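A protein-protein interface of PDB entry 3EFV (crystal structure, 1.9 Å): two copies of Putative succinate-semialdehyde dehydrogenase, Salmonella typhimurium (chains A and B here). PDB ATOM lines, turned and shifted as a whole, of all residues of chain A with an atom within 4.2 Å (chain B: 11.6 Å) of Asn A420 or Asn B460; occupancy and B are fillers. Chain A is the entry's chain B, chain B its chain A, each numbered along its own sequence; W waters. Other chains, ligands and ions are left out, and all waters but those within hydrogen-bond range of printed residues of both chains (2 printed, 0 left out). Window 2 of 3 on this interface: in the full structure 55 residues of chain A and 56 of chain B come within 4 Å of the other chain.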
ATOM      1  N   ILE A 397     -24.227   8.552  19.887  1.00  0.00           N
ATOM      2  CA  ILE A 397     -25.038   9.708  19.448  1.00  0.00           C
ATOM      3  C   ILE A 397     -26.217   9.946  20.407  1.00  0.00           C
ATOM      4  O   ILE A 397     -27.012   9.028  20.639  1.00  0.00           O
ATOM      5  CB  ILE A 397     -25.655   9.499  18.049  1.00  0.00           C
ATOM      6  CG1 ILE A 397     -24.624   8.974  17.048  1.00  0.00           C
ATOM      7  CG2 ILE A 397     -26.283  10.822  17.554  1.00  0.00           C
ATOM      8  CD1 ILE A 397     -25.269   8.358  15.767  1.00  0.00           C
ATOM      9  N   PHE A 398     -26.335  11.164  20.937  1.00  0.00           N
ATOM     10  CA  PHE A 398     -27.501  11.565  21.741  1.00  0.00           C
ATOM     11  C   PHE A 398     -28.361  12.527  20.931  1.00  0.00           C
ATOM     12  O   PHE A 398     -27.893  13.588  20.505  1.00  0.00           O
ATOM     13  CB  PHE A 398     -27.069  12.209  23.062  1.00  0.00           C
ATOM     14  CG  PHE A 398     -26.958  11.221  24.190  1.00  0.00           C
ATOM     15  CD1 PHE A 398     -25.842  10.392  24.299  1.00  0.00           C
ATOM     16  CD2 PHE A 398     -28.009  11.082  25.108  1.00  0.00           C
ATOM     17  CE1 PHE A 398     -25.744   9.428  25.318  1.00  0.00           C
ATOM     18  CE2 PHE A 398     -27.940  10.125  26.139  1.00  0.00           C
ATOM     19  CZ  PHE A 398     -26.802   9.299  26.251  1.00  0.00           C
ATOM     20  N   THR A 399     -29.600  12.127  20.685  1.00  0.00           N
ATOM     21  CA  THR A 399     -30.562  12.957  19.950  1.00  0.00           C
ATOM     22  C   THR A 399     -31.956  12.351  20.101  1.00  0.00           C
ATOM     23  O   THR A 399     -32.101  11.130  20.108  1.00  0.00           O
ATOM     24  CB  THR A 399     -30.211  13.060  18.428  1.00  0.00           C
ATOM     25  OG1 THR A 399     -31.196  13.854  17.750  1.00  0.00           O
ATOM     26  CG2 THR A 399     -30.149  11.678  17.746  1.00  0.00           C
ATOM     27  N   PHE A 418     -23.671   3.538  19.775  1.00  0.00           N
ATOM     28  CA  PHE A 418     -24.629   3.561  20.865  1.00  0.00           C
ATOM     29  C   PHE A 418     -25.502   4.793  20.736  1.00  0.00           C
ATOM     30  O   PHE A 418     -24.997   5.901  20.712  1.00  0.00           O
ATOM     31  CB  PHE A 418     -23.872   3.524  22.204  1.00  0.00           C
ATOM     32  CG  PHE A 418     -23.257   2.175  22.458  1.00  0.00           C
ATOM     33  CD1 PHE A 418     -23.932   1.226  23.225  1.00  0.00           C
ATOM     34  CD2 PHE A 418     -22.065   1.808  21.829  1.00  0.00           C
ATOM     35  CE1 PHE A 418     -23.394  -0.065  23.425  1.00  0.00           C
ATOM     36  CE2 PHE A 418     -21.514   0.517  22.022  1.00  0.00           C
ATOM     37  CZ  PHE A 418     -22.193  -0.420  22.828  1.00  0.00           C
ATOM     38  N   ILE A 419     -26.809   4.584  20.700  1.00  0.00           N
ATOM     39  CA  ILE A 419     -27.758   5.690  20.530  1.00  0.00           C
ATOM     40  C   ILE A 419     -28.442   5.934  21.877  1.00  0.00           C
ATOM     41  O   ILE A 419     -29.020   4.993  22.463  1.00  0.00           O
ATOM     42  CB  ILE A 419     -28.794   5.357  19.457  1.00  0.00           C
ATOM     43  CG1 ILE A 419     -28.112   5.195  18.073  1.00  0.00           C
ATOM     44  CG2 ILE A 419     -29.881   6.454  19.421  1.00  0.00           C
ATOM     45  CD1 ILE A 419     -29.020   4.560  17.014  1.00  0.00           C
ATOM     46  N   ASN A 420     -28.364   7.170  22.366  1.00  0.00           N
ATOM     47  CA  ASN A 420     -28.960   7.560  23.669  1.00  0.00           C
ATOM     48  C   ASN A 420     -28.678   6.589  24.822  1.00  0.00           C
ATOM     49  O   ASN A 420     -29.591   6.191  25.565  1.00  0.00           O
ATOM     50  CB  ASN A 420     -30.472   7.770  23.501  1.00  0.00           C
ATOM     51  CG  ASN A 420     -30.793   8.885  22.531  1.00  0.00           C
ATOM     52  OD1 ASN A 420     -30.130   9.922  22.551  1.00  0.00           O
ATOM     53  ND2 ASN A 420     -31.811   8.682  21.663  1.00  0.00           N
ATOM     54  N   GLY A 421     -27.416   6.175  24.953  1.00  0.00           N
ATOM     55  CA  GLY A 421     -27.037   5.304  26.063  1.00  0.00           C
ATOM     56  C   GLY A 421     -25.539   5.237  26.297  1.00  0.00           C
ATOM     57  O   GLY A 421     -24.770   6.025  25.738  1.00  0.00           O
ATOM     58  N   VAL B 115     -29.732  -9.355  23.248  1.00  0.00           N
ATOM     59  CA  VAL B 115     -30.100  -8.171  24.050  1.00  0.00           C
ATOM     60  C   VAL B 115     -31.624  -8.073  23.998  1.00  0.00           C
ATOM     61  O   VAL B 115     -32.225  -8.218  22.916  1.00  0.00           O
ATOM     62  CB  VAL B 115     -29.444  -6.885  23.503  1.00  0.00           C
ATOM     63  CG1 VAL B 115     -29.962  -5.633  24.242  1.00  0.00           C
ATOM     64  CG2 VAL B 115     -27.900  -6.994  23.609  1.00  0.00           C
ATOM     65  N   GLU B 116     -32.262  -7.854  25.150  1.00  0.00           N
ATOM     66  CA  GLU B 116     -33.721  -7.917  25.210  1.00  0.00           C
ATOM     67  C   GLU B 116     -34.424  -6.803  24.424  1.00  0.00           C
ATOM     68  O   GLU B 116     -33.909  -5.696  24.274  1.00  0.00           O
ATOM     69  CB  GLU B 116     -34.198  -7.888  26.667  1.00  0.00           C
ATOM     70  CG  GLU B 116     -33.850  -9.176  27.380  1.00  0.00           C
ATOM     71  CD  GLU B 116     -34.062  -9.133  28.878  1.00  0.00           C
ATOM     72  OE1 GLU B 116     -34.738  -8.208  29.390  1.00  0.00           O
ATOM     73  OE2 GLU B 116     -33.538 -10.061  29.539  1.00  0.00           O
ATOM     74  N   ASN B 117     -35.599  -7.137  23.899  1.00  0.00           N
ATOM     75  CA  ASN B 117     -36.551  -6.155  23.385  1.00  0.00           C
ATOM     76  C   ASN B 117     -36.075  -5.406  22.152  1.00  0.00           C
ATOM     77  O   ASN B 117     -36.387  -4.239  21.964  1.00  0.00           O
ATOM     78  CB  ASN B 117     -36.992  -5.169  24.490  1.00  0.00           C
ATOM     79  CG  ASN B 117     -38.292  -4.468  24.148  1.00  0.00           C
ATOM     80  OD1 ASN B 117     -39.120  -5.024  23.430  1.00  0.00           O
ATOM     81  ND2 ASN B 117     -38.471  -3.244  24.636  1.00  0.00           N
ATOM     82  N   GLN B 118     -35.299  -6.101  21.329  1.00  0.00           N
ATOM     83  CA  GLN B 118     -34.856  -5.599  20.026  1.00  0.00           C
ATOM     84  C   GLN B 118     -34.091  -4.271  20.165  1.00  0.00           C
ATOM     85  O   GLN B 118     -34.237  -3.361  19.334  1.00  0.00           O
ATOM     86  CB  GLN B 118     -36.051  -5.495  19.050  1.00  0.00           C
ATOM     87  CG  GLN B 118     -36.746  -6.842  18.765  1.00  0.00           C
ATOM     88  CD  GLN B 118     -37.695  -7.303  19.872  1.00  0.00           C
ATOM     89  OE1 GLN B 118     -38.486  -6.513  20.381  1.00  0.00           O
ATOM     90  NE2 GLN B 118     -37.630  -8.591  20.235  1.00  0.00           N
ATOM     91  N   GLN B 119     -33.268  -4.154  21.211  1.00  0.00           N
ATOM     92  CA  GLN B 119     -32.562  -2.885  21.431  1.00  0.00           C
ATOM     93  C   GLN B 119     -31.189  -2.832  20.739  1.00  0.00           C
ATOM     94  O   GLN B 119     -30.616  -1.746  20.592  1.00  0.00           O
ATOM     95  CB  GLN B 119     -32.391  -2.595  22.926  1.00  0.00           C
ATOM     96  CG  GLN B 119     -33.738  -2.484  23.694  1.00  0.00           C
ATOM     97  CD  GLN B 119     -34.543  -1.263  23.325  1.00  0.00           C
ATOM     98  OE1 GLN B 119     -35.517  -1.346  22.565  1.00  0.00           O
ATOM     99  NE2 GLN B 119     -34.162  -0.131  23.860  1.00  0.00           N
ATOM    100  N   ALA B 120     -30.684  -3.987  20.325  1.00  0.00           N
ATOM    101  CA  ALA B 120     -29.358  -4.074  19.660  1.00  0.00           C
ATOM    102  C   ALA B 120     -29.390  -5.029  18.477  1.00  0.00           C
ATOM    103  O   ALA B 120     -29.955  -6.134  18.562  1.00  0.00           O
ATOM    104  CB  ALA B 120     -28.246  -4.497  20.674  1.00  0.00           C
ATOM    105  N   VAL B 121     -28.809  -4.587  17.361  1.00  0.00           N
ATOM    106  CA  VAL B 121     -28.706  -5.423  16.182  1.00  0.00           C
ATOM    107  C   VAL B 121     -27.264  -5.400  15.700  1.00  0.00           C
ATOM    108  O   VAL B 121     -26.498  -4.507  16.069  1.00  0.00           O
ATOM    109  CB  VAL B 121     -29.585  -4.892  15.009  1.00  0.00           C
ATOM    110  CG1 VAL B 121     -31.076  -5.037  15.325  1.00  0.00           C
ATOM    111  CG2 VAL B 121     -29.223  -3.441  14.649  1.00  0.00           C
ATOM    112  N   THR B 456     -22.109  -3.198  15.572  1.00  0.00           N
ATOM    113  CA  THR B 456     -23.167  -3.288  16.597  1.00  0.00           C
ATOM    114  C   THR B 456     -23.882  -1.934  16.675  1.00  0.00           C
ATOM    115  O   THR B 456     -23.226  -0.887  16.780  1.00  0.00           O
ATOM    116  CB  THR B 456     -22.532  -3.602  17.961  1.00  0.00           C
ATOM    117  OG1 THR B 456     -22.008  -4.936  17.920  1.00  0.00           O
ATOM    118  CG2 THR B 456     -23.594  -3.499  19.107  1.00  0.00           C
ATOM    119  N   VAL B 457     -25.215  -1.934  16.618  1.00  0.00           N
ATOM    120  CA  VAL B 457     -25.978  -0.716  16.868  1.00  0.00           C
ATOM    121  C   VAL B 457     -26.929  -0.968  18.033  1.00  0.00           C
ATOM    122  O   VAL B 457     -27.797  -1.832  17.937  1.00  0.00           O
ATOM    123  CB  VAL B 457     -26.792  -0.279  15.612  1.00  0.00           C
ATOM    124  CG1 VAL B 457     -27.478   1.082  15.888  1.00  0.00           C
ATOM    125  CG2 VAL B 457     -25.859  -0.139  14.403  1.00  0.00           C
ATOM    126  N   TRP B 458     -26.738  -0.252  19.134  1.00  0.00           N
ATOM    127  CA  TRP B 458     -27.473  -0.534  20.374  1.00  0.00           C
ATOM    128  C   TRP B 458     -28.108   0.751  20.879  1.00  0.00           C
ATOM    129  O   TRP B 458     -27.407   1.720  21.187  1.00  0.00           O
ATOM    130  CB  TRP B 458     -26.481  -1.071  21.409  1.00  0.00           C
ATOM    131  CG  TRP B 458     -27.056  -1.716  22.639  1.00  0.00           C
ATOM    132  CD1 TRP B 458     -28.296  -1.508  23.204  1.00  0.00           C
ATOM    133  CD2 TRP B 458     -26.371  -2.631  23.487  1.00  0.00           C
ATOM    134  NE1 TRP B 458     -28.409  -2.255  24.364  1.00  0.00           N
ATOM    135  CE2 TRP B 458     -27.248  -2.966  24.547  1.00  0.00           C
ATOM    136  CE3 TRP B 458     -25.098  -3.224  23.449  1.00  0.00           C
ATOM    137  CZ2 TRP B 458     -26.888  -3.871  25.561  1.00  0.00           C
ATOM    138  CZ3 TRP B 458     -24.736  -4.110  24.473  1.00  0.00           C
ATOM    139  CH2 TRP B 458     -25.628  -4.420  25.507  1.00  0.00           C
ATOM    140  N   LYS B 459     -29.430   0.785  20.965  1.00  0.00           N
ATOM    141  CA  LYS B 459     -30.094   1.995  21.464  1.00  0.00           C
ATOM    142  C   LYS B 459     -30.515   1.833  22.937  1.00  0.00           C
ATOM    143  O   LYS B 459     -30.844   0.711  23.373  1.00  0.00           O
ATOM    144  CB  LYS B 459     -31.303   2.364  20.598  1.00  0.00           C
ATOM    145  CG  LYS B 459     -32.369   1.285  20.550  1.00  0.00           C
ATOM    146  CD  LYS B 459     -33.558   1.701  19.657  1.00  0.00           C
ATOM    147  CE  LYS B 459     -34.524   0.532  19.543  1.00  0.00           C
ATOM    148  NZ  LYS B 459     -35.746   0.892  18.751  1.00  0.00           N
ATOM    149  N   ASN B 460     -30.511   2.948  23.670  1.00  0.00           N
ATOM    150  CA  ASN B 460     -31.066   3.011  25.047  1.00  0.00           C
ATOM    151  C   ASN B 460     -30.361   2.059  26.010  1.00  0.00           C
ATOM    152  O   ASN B 460     -31.013   1.437  26.865  1.00  0.00           O
ATOM    153  CB  ASN B 460     -32.582   2.717  25.041  1.00  0.00           C
ATOM    154  CG  ASN B 460     -33.330   3.533  23.990  1.00  0.00           C
ATOM    155  OD1 ASN B 460     -33.099   4.744  23.849  1.00  0.00           O
ATOM    156  ND2 ASN B 460     -34.216   2.878  23.240  1.00  0.00           N
ATOM    157  N   ARG B 461     -29.045   1.902  25.869  1.00  0.00           N
ATOM    158  CA  ARG B 461     -28.344   1.051  26.831  1.00  0.00           C
ATOM    159  C   ARG B 461     -28.112   1.874  28.101  1.00  0.00           C
ATOM    160  O   ARG B 461     -27.221   2.724  28.162  1.00  0.00           O
ATOM    161  CB  ARG B 461     -27.026   0.501  26.262  1.00  0.00           C
ATOM    162  CG  ARG B 461     -26.392  -0.499  27.225  1.00  0.00           C
ATOM    163  CD  ARG B 461     -25.028  -1.038  26.775  1.00  0.00           C
ATOM    164  NE  ARG B 461     -24.477  -1.862  27.854  1.00  0.00           N
ATOM    165  CZ  ARG B 461     -23.811  -1.387  28.912  1.00  0.00           C
ATOM    166  NH1 ARG B 461     -23.550  -0.077  29.031  1.00  0.00           N
ATOM    167  NH2 ARG B 461     -23.383  -2.224  29.845  1.00  0.00           N
ATOM    168  N   VAL B 462     -28.953   1.649  29.108  1.00  0.00           N
ATOM    169  CA  VAL B 462     -28.866   2.403  30.365  1.00  0.00           C
ATOM    170  C   VAL B 462     -29.078   1.421  31.516  1.00  0.00           C
ATOM    171  O   VAL B 462     -30.061   0.655  31.474  1.00  0.00           O
ATOM    172  CB  VAL B 462     -29.935   3.525  30.454  1.00  0.00           C
ATOM    173  CG1 VAL B 462     -29.825   4.266  31.802  1.00  0.00           C
ATOM    174  CG2 VAL B 462     -29.818   4.528  29.307  1.00  0.00           C
HETATM  175  O   HOH W   1     -32.322   6.398  26.135  1.00  0.00           O
HETATM  176  O   HOH W   2     -33.341   6.240  21.677  1.00  0.00           O
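Water W2 lies within hydrogen-bond range of OD1 of Asn B460 (2.6 Å) and ND2 of Asn A420 (2.9 Å).
Water W1 lies within hydrogen-bond range of the backbone carbonyl oxygen of Asn A420 (2.8 Å) and the side-chain amide oxygen of Asn B460 (2.9 Å).
O of Thr A399 lies within hydrogen-bond range of ND2 of Asn A420.
The side-chain amide nitrogen (ND2) of Asn B460 sits close to the side-chain amide nitrogen (NE2) of Gln B119 (3.1 Å).
The backbone NH (N) of Lys B459 lies within hydrogen-bond range of the backbone carbonyl oxygen (O) of Gln B119.
O of Ile A397 is in hydrogen-bond range of N of Asn A420, at 2.9 Å.
O of Val B121 is in hydrogen-bond range of N of Val B457.
N of Ile A397 sits at hydrogen-bond distance from O of Phe A418, 2.9 Å away.
Hydrophobic or aromatic side chains of chain B within 4 Å of the printed part of chain A: Val B457 and Trp B458.
Of the 7 printed residues of chain A, 4 touch a printed residue of chain B.
Hydrophobic or aromatic side chains of chain A within 4 Å of the printed part of chain B: Phe A418 and Ile A419.
Among the printed residues, no Asp or Glu carboxylate lies within 4 Å of a Lys or Arg side-chain nitrogen of the other chain.
No position is printed for both chains.
Of the 8 pairs that touch across the chains among the printed residues, none has its exchanged pair printed and touching as well.
The backbone carbonyl oxygen (O) of Ile A419 is in hydrogen-bond range of the backbone NH (N) of Asn B460, at 2.8 Å.
O of Trp B458 is in hydrogen-bond range of N of Ile A419, 3.0 Å away.
No residue of chain B comes within 4 Å of Thr A399.
Printed residues of chain B within 4 Å of Phe A418: Trp B458 and Arg B461.
Of chain B, only Asn B460 (3.5 Å) comes within 4 Å of Asn A420.
Of the printed residues of chain A, Val B457 touches Ile A419.
Printed residues of chain A within 4 Å of Trp B458: Phe A418 and Ile A419.
Asn B460 touches two residues of chain A.
Of the printed residues of chain A, Arg B461 touches Phe A418 and Gly A421.
The nearest printed residue of chain A that does not touch Asn B460 is Gly A421 (4.6 Å).
Among the printed residues, merely in contact across the chains: Gly A421 with Arg B461 (3.3 Å), Ile A419 with Lys B459 (3.3 Å), Phe A418 with Trp B458 (3.3 Å), Asn A420 with Asn B460 (3.5 Å), Phe A418 with Arg B461 (3.9 Å) and Ile A419 with Val B457 (3.97 Å).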
